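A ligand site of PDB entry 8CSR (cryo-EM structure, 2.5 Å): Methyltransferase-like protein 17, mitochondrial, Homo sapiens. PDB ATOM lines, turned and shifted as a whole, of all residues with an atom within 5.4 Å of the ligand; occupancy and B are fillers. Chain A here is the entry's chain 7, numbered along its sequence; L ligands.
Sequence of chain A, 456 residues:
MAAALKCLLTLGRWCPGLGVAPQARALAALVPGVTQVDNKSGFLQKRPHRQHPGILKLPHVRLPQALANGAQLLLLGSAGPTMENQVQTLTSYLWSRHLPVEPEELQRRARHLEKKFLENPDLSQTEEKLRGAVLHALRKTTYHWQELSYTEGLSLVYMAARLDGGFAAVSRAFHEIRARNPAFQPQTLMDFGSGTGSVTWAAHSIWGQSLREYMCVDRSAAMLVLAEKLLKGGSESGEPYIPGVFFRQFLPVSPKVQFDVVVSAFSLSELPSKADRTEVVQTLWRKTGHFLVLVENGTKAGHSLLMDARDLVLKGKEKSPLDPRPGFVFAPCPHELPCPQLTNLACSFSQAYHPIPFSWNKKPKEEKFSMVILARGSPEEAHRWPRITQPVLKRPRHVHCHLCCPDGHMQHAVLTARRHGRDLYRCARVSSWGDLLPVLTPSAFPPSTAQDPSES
The backbone carbonyl oxygen (O) of Arg 219 is in hydrogen-bond range of the side-chain amide nitrogen (NE2) of Gln 249, 2.9 Å away.
The side-chain carboxylate (OE2) of Glu 270 lies within hydrogen-bond range of the side-chain hydroxyl (OH) of Tyr 150 (2.8 Å).
OG1 of Thr 196 lies within hydrogen-bond range of OG of Ser 198, 3.2 Å away.
O of Tyr 150 sits at hydrogen-bond distance from OG of Ser 220 (2.8 Å).
The side-chain hydroxyl (OG) of Ser 267 lies within hydrogen-bond range of the backbone carbonyl oxygen (O) of Gly 193 (3.1 Å).
The side-chain carboxylate (OD2) of Asp 218 is in hydrogen-bond range of the backbone NH (N) of Ser 220, at 3.2 Å.
The backbone carbonyl oxygen (O) of Ala 265 lies within hydrogen-bond range of the side-chain hydroxyl (OG) of Ser 267 (3.3 Å).
The backbone NH (N) of Met 223 lies within hydrogen-bond range of the side-chain hydroxyl (OG) of Ser 220, 3.5 Å away.
N1 of the ligand lies close to O of Ala 265 (2.5 Å).
N6 of the ligand sits close to N of Arg 219 (3.4 Å).
OD1 of Asp 218 sits close to O4 of the ligand, at 2.5 Å.
O2 of the ligand sits close to OG1 of Thr 196.
The side-chain hydroxyl (OG) of Ser 198 sits close to an oxygen (O2) of the ligand.
The backbone carbonyl oxygen (O) of Gly 193 lies close to a nitrogen (N1) of the ligand (3.1 Å).
Tyr 150 touches the ligand (OH to C5, 3.99 Å).
Tyr 158 touches the ligand (OH to C5, 3.2 Å).
CE1 of Phe 192 touches C14 of the ligand, 3.5 Å away.
Gly 195 touches the ligand (N to C1, 3.7 Å).
Ser 220 touches the ligand.
Met 223 touches the ligand.
Phe 266 touches the ligand.
Ser 267 touches the ligand.
Glu 270 touches the ligand.
Leu 271 touches the ligand.
Along chain A the residues within 4 Å of the ligand span positions 150 to 271.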
ATOM      1  N   TYR A 150     -22.605   7.199  21.736  1.00  0.00           N
ATOM      2  CA  TYR A 150     -22.485   8.393  22.580  1.00  0.00           C
ATOM      3  C   TYR A 150     -23.268   9.521  21.937  1.00  0.00           C
ATOM      4  O   TYR A 150     -22.733  10.301  21.144  1.00  0.00           O
ATOM      5  CB  TYR A 150     -21.026   8.762  22.778  1.00  0.00           C
ATOM      6  CG  TYR A 150     -20.334   7.895  23.800  1.00  0.00           C
ATOM      7  CD1 TYR A 150     -20.454   8.149  25.153  1.00  0.00           C
ATOM      8  CD2 TYR A 150     -19.552   6.823  23.409  1.00  0.00           C
ATOM      9  CE1 TYR A 150     -19.829   7.358  26.094  1.00  0.00           C
ATOM     10  CE2 TYR A 150     -18.911   6.022  24.327  1.00  0.00           C
ATOM     11  CZ  TYR A 150     -19.055   6.292  25.672  1.00  0.00           C
ATOM     12  OH  TYR A 150     -18.428   5.506  26.600  1.00  0.00           O
ATOM     13  N   TYR A 158     -21.356  10.933  30.532  1.00  0.00           N
ATOM     14  CA  TYR A 158     -19.946  10.541  30.534  1.00  0.00           C
ATOM     15  C   TYR A 158     -19.074  11.669  31.063  1.00  0.00           C
ATOM     16  O   TYR A 158     -18.159  11.423  31.862  1.00  0.00           O
ATOM     17  CB  TYR A 158     -19.505  10.153  29.118  1.00  0.00           C
ATOM     18  CG  TYR A 158     -18.115   9.565  29.104  1.00  0.00           C
ATOM     19  CD1 TYR A 158     -17.932   8.201  29.256  1.00  0.00           C
ATOM     20  CD2 TYR A 158     -17.011  10.371  28.954  1.00  0.00           C
ATOM     21  CE1 TYR A 158     -16.669   7.659  29.251  1.00  0.00           C
ATOM     22  CE2 TYR A 158     -15.742   9.842  28.947  1.00  0.00           C
ATOM     23  CZ  TYR A 158     -15.575   8.484  29.098  1.00  0.00           C
ATOM     24  OH  TYR A 158     -14.309   7.950  29.104  1.00  0.00           O
ATOM     25  N   ARG A 162     -16.538  10.875  34.095  1.00  0.00           N
ATOM     26  CA  ARG A 162     -15.167  10.506  33.760  1.00  0.00           C
ATOM     27  C   ARG A 162     -14.261  11.683  33.444  1.00  0.00           C
ATOM     28  O   ARG A 162     -13.058  11.474  33.292  1.00  0.00           O
ATOM     29  CB  ARG A 162     -15.167   9.547  32.572  1.00  0.00           C
ATOM     30  CG  ARG A 162     -15.960   8.256  32.800  1.00  0.00           C
ATOM     31  CD  ARG A 162     -15.282   7.310  33.777  1.00  0.00           C
ATOM     32  NE  ARG A 162     -13.895   7.052  33.407  1.00  0.00           N
ATOM     33  CZ  ARG A 162     -12.862   7.064  34.227  1.00  0.00           C
ATOM     34  NH1 ARG A 162     -12.993   7.275  35.525  1.00  0.00           N
ATOM     35  NH2 ARG A 162     -11.641   6.862  33.738  1.00  0.00           N
ATOM     36  N   GLY A 166     -10.742  10.780  34.340  1.00  0.00           N
ATOM     37  CA  GLY A 166      -9.856  10.626  33.202  1.00  0.00           C
ATOM     38  C   GLY A 166      -8.714  11.628  33.210  1.00  0.00           C
ATOM     39  O   GLY A 166      -7.582  11.299  32.857  1.00  0.00           O
ATOM     40  N   VAL A 170      -4.459  10.675  33.136  1.00  0.00           N
ATOM     41  CA  VAL A 170      -3.575  11.136  32.074  1.00  0.00           C
ATOM     42  C   VAL A 170      -2.525  12.086  32.623  1.00  0.00           C
ATOM     43  O   VAL A 170      -1.376  12.104  32.160  1.00  0.00           O
ATOM     44  CB  VAL A 170      -4.388  11.780  30.943  1.00  0.00           C
ATOM     45  CG1 VAL A 170      -3.460  12.264  29.844  1.00  0.00           C
ATOM     46  CG2 VAL A 170      -5.393  10.794  30.377  1.00  0.00           C
ATOM     47  N   ASP A 191      -4.652  12.920  19.868  1.00  0.00           N
ATOM     48  CA  ASP A 191      -5.457  12.231  20.865  1.00  0.00           C
ATOM     49  C   ASP A 191      -6.536  11.421  20.158  1.00  0.00           C
ATOM     50  O   ASP A 191      -7.577  11.971  19.774  1.00  0.00           O
ATOM     51  CB  ASP A 191      -6.065  13.211  21.845  1.00  0.00           C
ATOM     52  CG  ASP A 191      -6.941  12.524  22.872  1.00  0.00           C
ATOM     53  OD1 ASP A 191      -8.152  12.808  22.895  1.00  0.00           O
ATOM     54  OD2 ASP A 191      -6.416  11.693  23.647  1.00  0.00           O
ATOM     55  N   PHE A 192      -6.290  10.132  19.976  1.00  0.00           N
ATOM     56  CA  PHE A 192      -7.331   9.248  19.474  1.00  0.00           C
ATOM     57  C   PHE A 192      -8.389   9.044  20.545  1.00  0.00           C
ATOM     58  O   PHE A 192      -8.071   8.946  21.736  1.00  0.00           O
ATOM     59  CB  PHE A 192      -6.736   7.914  19.045  1.00  0.00           C
ATOM     60  CG  PHE A 192      -7.764   6.915  18.584  1.00  0.00           C
ATOM     61  CD1 PHE A 192      -8.320   7.023  17.326  1.00  0.00           C
ATOM     62  CD2 PHE A 192      -8.158   5.881  19.401  1.00  0.00           C
ATOM     63  CE1 PHE A 192      -9.267   6.114  16.906  1.00  0.00           C
ATOM     64  CE2 PHE A 192      -9.104   4.971  18.981  1.00  0.00           C
ATOM     65  CZ  PHE A 192      -9.659   5.088  17.733  1.00  0.00           C
ATOM     66  N   GLY A 193      -9.641   8.988  20.132  1.00  0.00           N
ATOM     67  CA  GLY A 193     -10.720   8.843  21.080  1.00  0.00           C
ATOM     68  C   GLY A 193     -10.796  10.039  22.017  1.00  0.00           C
ATOM     69  O   GLY A 193     -10.663   9.889  23.233  1.00  0.00           O
ATOM     70  N   SER A 194     -10.992  11.217  21.448  1.00  0.00           N
ATOM     71  CA  SER A 194     -11.114  12.457  22.206  1.00  0.00           C
ATOM     72  C   SER A 194     -12.577  12.670  22.537  1.00  0.00           C
ATOM     73  O   SER A 194     -13.336  13.275  21.778  1.00  0.00           O
ATOM     74  CB  SER A 194     -10.563  13.623  21.401  1.00  0.00           C
ATOM     75  OG  SER A 194     -11.378  13.848  20.259  1.00  0.00           O
ATOM     76  N   GLY A 195     -12.988  12.186  23.700  1.00  0.00           N
ATOM     77  CA  GLY A 195     -14.372  12.317  24.105  1.00  0.00           C
ATOM     78  C   GLY A 195     -14.708  13.687  24.651  1.00  0.00           C
ATOM     79  O   GLY A 195     -15.510  14.416  24.069  1.00  0.00           O
ATOM     80  N   THR A 196     -14.079  14.046  25.776  1.00  0.00           N
ATOM     81  CA  THR A 196     -14.338  15.311  26.443  1.00  0.00           C
ATOM     82  C   THR A 196     -13.126  16.238  26.449  1.00  0.00           C
ATOM     83  O   THR A 196     -13.194  17.307  27.056  1.00  0.00           O
ATOM     84  CB  THR A 196     -14.788  15.066  27.882  1.00  0.00           C
ATOM     85  OG1 THR A 196     -13.843  14.216  28.556  1.00  0.00           O
ATOM     86  CG2 THR A 196     -16.155  14.417  27.910  1.00  0.00           C
ATOM     87  N   GLY A 197     -12.030  15.854  25.810  1.00  0.00           N
ATOM     88  CA  GLY A 197     -10.856  16.700  25.750  1.00  0.00           C
ATOM     89  C   GLY A 197      -9.978  16.656  26.974  1.00  0.00           C
ATOM     90  O   GLY A 197      -9.153  17.560  27.151  1.00  0.00           O
ATOM     91  N   SER A 198     -10.127  15.634  27.820  1.00  0.00           N
ATOM     92  CA  SER A 198      -9.330  15.575  29.043  1.00  0.00           C
ATOM     93  C   SER A 198      -7.840  15.548  28.735  1.00  0.00           C
ATOM     94  O   SER A 198      -7.035  16.154  29.449  1.00  0.00           O
ATOM     95  CB  SER A 198      -9.728  14.357  29.859  1.00  0.00           C
ATOM     96  OG  SER A 198     -11.097  14.406  30.225  1.00  0.00           O
ATOM     97  N   VAL A 199      -7.465  14.829  27.682  1.00  0.00           N
ATOM     98  CA  VAL A 199      -6.050  14.752  27.310  1.00  0.00           C
ATOM     99  C   VAL A 199      -5.536  16.128  26.894  1.00  0.00           C
ATOM    100  O   VAL A 199      -4.426  16.520  27.256  1.00  0.00           O
ATOM    101  CB  VAL A 199      -5.856  13.717  26.187  1.00  0.00           C
ATOM    102  CG1 VAL A 199      -4.397  13.663  25.778  1.00  0.00           C
ATOM    103  CG2 VAL A 199      -6.355  12.371  26.631  1.00  0.00           C
ATOM    104  N   VAL A 217      -9.366  13.363  17.745  1.00  0.00           N
ATOM    105  CA  VAL A 217     -10.150  12.483  16.869  1.00  0.00           C
ATOM    106  C   VAL A 217     -11.208  11.793  17.701  1.00  0.00           C
ATOM    107  O   VAL A 217     -10.930  11.317  18.804  1.00  0.00           O
ATOM    108  CB  VAL A 217      -9.251  11.443  16.165  1.00  0.00           C
ATOM    109  CG1 VAL A 217     -10.087  10.565  15.262  1.00  0.00           C
ATOM    110  CG2 VAL A 217      -8.154  12.133  15.380  1.00  0.00           C
ATOM    111  N   ASP A 218     -12.431  11.753  17.179  1.00  0.00           N
ATOM    112  CA  ASP A 218     -13.538  11.088  17.855  1.00  0.00           C
ATOM    113  C   ASP A 218     -14.675  10.929  16.863  1.00  0.00           C
ATOM    114  O   ASP A 218     -15.079  11.911  16.228  1.00  0.00           O
ATOM    115  CB  ASP A 218     -13.995  11.891  19.070  1.00  0.00           C
ATOM    116  CG  ASP A 218     -14.982  11.138  19.936  1.00  0.00           C
ATOM    117  OD1 ASP A 218     -14.532  10.297  20.743  1.00  0.00           O
ATOM    118  OD2 ASP A 218     -16.196  11.375  19.805  1.00  0.00           O
ATOM    119  N   ARG A 219     -15.199   9.707  16.726  1.00  0.00           N
ATOM    120  CA  ARG A 219     -16.206   9.457  15.695  1.00  0.00           C
ATOM    121  C   ARG A 219     -17.559  10.058  16.027  1.00  0.00           C
ATOM    122  O   ARG A 219     -18.367  10.266  15.125  1.00  0.00           O
ATOM    123  CB  ARG A 219     -16.391   7.951  15.472  1.00  0.00           C
ATOM    124  CG  ARG A 219     -16.924   7.183  16.673  1.00  0.00           C
ATOM    125  CD  ARG A 219     -17.053   5.703  16.373  1.00  0.00           C
ATOM    126  NE  ARG A 219     -18.082   5.437  15.377  1.00  0.00           N
ATOM    127  CZ  ARG A 219     -18.218   4.283  14.734  1.00  0.00           C
ATOM    128  NH1 ARG A 219     -17.417   3.258  14.965  1.00  0.00           N
ATOM    129  NH2 ARG A 219     -19.179   4.165  13.826  1.00  0.00           N
ATOM    130  N   SER A 220     -17.830  10.353  17.298  1.00  0.00           N
ATOM    131  CA  SER A 220     -19.136  10.840  17.710  1.00  0.00           C
ATOM    132  C   SER A 220     -19.204  12.340  17.499  1.00  0.00           C
ATOM    133  O   SER A 220     -18.321  13.081  17.955  1.00  0.00           O
ATOM    134  CB  SER A 220     -19.391  10.496  19.177  1.00  0.00           C
ATOM    135  OG  SER A 220     -20.569  11.116  19.639  1.00  0.00           O
ATOM    136  N   MET A 223     -19.825  14.221  21.025  1.00  0.00           N
ATOM    137  CA  MET A 223     -18.650  14.396  21.879  1.00  0.00           C
ATOM    138  C   MET A 223     -17.773  15.529  21.366  1.00  0.00           C
ATOM    139  O   MET A 223     -17.229  16.302  22.167  1.00  0.00           O
ATOM    140  CB  MET A 223     -17.855  13.091  21.939  1.00  0.00           C
ATOM    141  CG  MET A 223     -18.399  12.101  22.942  1.00  0.00           C
ATOM    142  SD  MET A 223     -17.968  12.509  24.633  1.00  0.00           S
ATOM    143  CE  MET A 223     -18.102  10.902  25.387  1.00  0.00           C
ATOM    144  N   GLN A 249     -13.249  13.737  12.786  1.00  0.00           N
ATOM    145  CA  GLN A 249     -14.114  12.588  13.044  1.00  0.00           C
ATOM    146  C   GLN A 249     -13.492  11.274  12.612  1.00  0.00           C
ATOM    147  O   GLN A 249     -13.941  10.219  13.074  1.00  0.00           O
ATOM    148  CB  GLN A 249     -15.473  12.778  12.353  1.00  0.00           C
ATOM    149  CG  GLN A 249     -16.487  11.694  12.683  1.00  0.00           C
ATOM    150  CD  GLN A 249     -17.844  11.945  12.090  1.00  0.00           C
ATOM    151  OE1 GLN A 249     -18.068  12.948  11.419  1.00  0.00           O
ATOM    152  NE2 GLN A 249     -18.776  11.029  12.326  1.00  0.00           N
ATOM    153  N   ALA A 265      -6.582   7.392  25.717  1.00  0.00           N
ATOM    154  CA  ALA A 265      -6.996   7.224  27.106  1.00  0.00           C
ATOM    155  C   ALA A 265      -8.418   6.676  27.140  1.00  0.00           C
ATOM    156  O   ALA A 265      -9.361   7.359  26.732  1.00  0.00           O
ATOM    157  CB  ALA A 265      -6.910   8.562  27.853  1.00  0.00           C
ATOM    158  N   PHE A 266      -8.567   5.461  27.655  1.00  0.00           N
ATOM    159  CA  PHE A 266      -9.871   4.852  27.893  1.00  0.00           C
ATOM    160  C   PHE A 266     -10.687   4.769  26.611  1.00  0.00           C
ATOM    161  O   PHE A 266     -11.911   4.938  26.608  1.00  0.00           O
ATOM    162  CB  PHE A 266     -10.639   5.620  28.964  1.00  0.00           C
ATOM    163  CG  PHE A 266      -9.839   5.903  30.202  1.00  0.00           C
ATOM    164  CD1 PHE A 266      -9.715   4.947  31.194  1.00  0.00           C
ATOM    165  CD2 PHE A 266      -9.185   7.114  30.366  1.00  0.00           C
ATOM    166  CE1 PHE A 266      -8.981   5.208  32.318  1.00  0.00           C
ATOM    167  CE2 PHE A 266      -8.448   7.366  31.488  1.00  0.00           C
ATOM    168  CZ  PHE A 266      -8.345   6.417  32.470  1.00  0.00           C
ATOM    169  N   SER A 267     -10.007   4.480  25.504  1.00  0.00           N
ATOM    170  CA  SER A 267     -10.631   4.466  24.182  1.00  0.00           C
ATOM    171  C   SER A 267     -10.493   3.134  23.466  1.00  0.00           C
ATOM    172  O   SER A 267     -11.411   2.743  22.744  1.00  0.00           O
ATOM    173  CB  SER A 267     -10.035   5.573  23.322  1.00  0.00           C
ATOM    174  OG  SER A 267     -10.521   6.841  23.716  1.00  0.00           O
ATOM    175  N   GLU A 270     -13.362   0.628  23.783  1.00  0.00           N
ATOM    176  CA  GLU A 270     -14.614   0.847  23.065  1.00  0.00           C
ATOM    177  C   GLU A 270     -14.623   0.252  21.668  1.00  0.00           C
ATOM    178  O   GLU A 270     -15.664   0.248  21.016  1.00  0.00           O
ATOM    179  CB  GLU A 270     -14.911   2.344  22.968  1.00  0.00           C
ATOM    180  CG  GLU A 270     -14.906   3.085  24.299  1.00  0.00           C
ATOM    181  CD  GLU A 270     -16.249   3.062  25.005  1.00  0.00           C
ATOM    182  OE1 GLU A 270     -17.187   2.392  24.506  1.00  0.00           O
ATOM    183  OE2 GLU A 270     -16.375   3.704  26.067  1.00  0.00           O
ATOM    184  N   LEU A 271     -13.483  -0.246  21.191  1.00  0.00           N
ATOM    185  CA  LEU A 271     -13.402  -0.798  19.860  1.00  0.00           C
ATOM    186  C   LEU A 271     -14.023  -2.195  19.825  1.00  0.00           C
ATOM    187  O   LEU A 271     -13.881  -2.955  20.787  1.00  0.00           O
ATOM    188  CB  LEU A 271     -11.950  -0.864  19.408  1.00  0.00           C
ATOM    189  CG  LEU A 271     -11.269   0.493  19.253  1.00  0.00           C
ATOM    190  CD1 LEU A 271      -9.799   0.333  18.934  1.00  0.00           C
ATOM    191  CD2 LEU A 271     -11.938   1.309  18.166  1.00  0.00           C
HETATM  192  N1  LIG L   1     -10.176   9.677  26.240  1.00  0.00           N
HETATM  193  C1  LIG L   1     -11.381  10.419  26.577  1.00  0.00           C
HETATM  194  C2  LIG L   1     -11.222  11.192  27.877  1.00  0.00           C
HETATM  195  O1  LIG L   1     -10.201  11.108  28.556  1.00  0.00           O
HETATM  196  O2  LIG L   1     -12.114  11.938  28.271  1.00  0.00           O
HETATM  197  C3  LIG L   1     -12.577   9.480  26.677  1.00  0.00           C
HETATM  198  C4  LIG L   1     -12.589   8.294  25.723  1.00  0.00           C
HETATM  199  S1  LIG L   1     -14.284   7.820  25.284  1.00  0.00           S
HETATM  200  C5  LIG L   1     -14.534   6.352  26.317  1.00  0.00           C
HETATM  201  C6  LIG L   1     -14.011   6.994  23.699  1.00  0.00           C
HETATM  202  C7  LIG L   1     -14.347   7.829  22.473  1.00  0.00           C
HETATM  203  O3  LIG L   1     -13.832   7.176  21.330  1.00  0.00           O
HETATM  204  C8  LIG L   1     -15.843   7.968  22.268  1.00  0.00           C
HETATM  205  O4  LIG L   1     -16.209   9.332  22.272  1.00  0.00           O
HETATM  206  C9  LIG L   1     -16.135   7.337  20.932  1.00  0.00           C
HETATM  207  O5  LIG L   1     -17.018   8.131  20.170  1.00  0.00           O
HETATM  208  C10 LIG L   1     -14.760   7.215  20.276  1.00  0.00           C
HETATM  209  N2  LIG L   1     -14.624   6.038  19.374  1.00  0.00           N
HETATM  210  C11 LIG L   1     -15.102   4.771  19.545  1.00  0.00           C
HETATM  211  N3  LIG L   1     -14.744   4.026  18.487  1.00  0.00           N
HETATM  212  C12 LIG L   1     -14.036   4.788  17.637  1.00  0.00           C
HETATM  213  C13 LIG L   1     -13.433   4.527  16.415  1.00  0.00           C
HETATM  214  N4  LIG L   1     -13.516   3.316  15.886  1.00  0.00           N
HETATM  215  N5  LIG L   1     -12.754   5.532  15.753  1.00  0.00           N
HETATM  216  C14 LIG L   1     -12.675   6.788  16.311  1.00  0.00           C
HETATM  217  N6  LIG L   1     -13.275   7.040  17.530  1.00  0.00           N
HETATM  218  C15 LIG L   1     -13.949   6.062  18.179  1.00  0.00           C
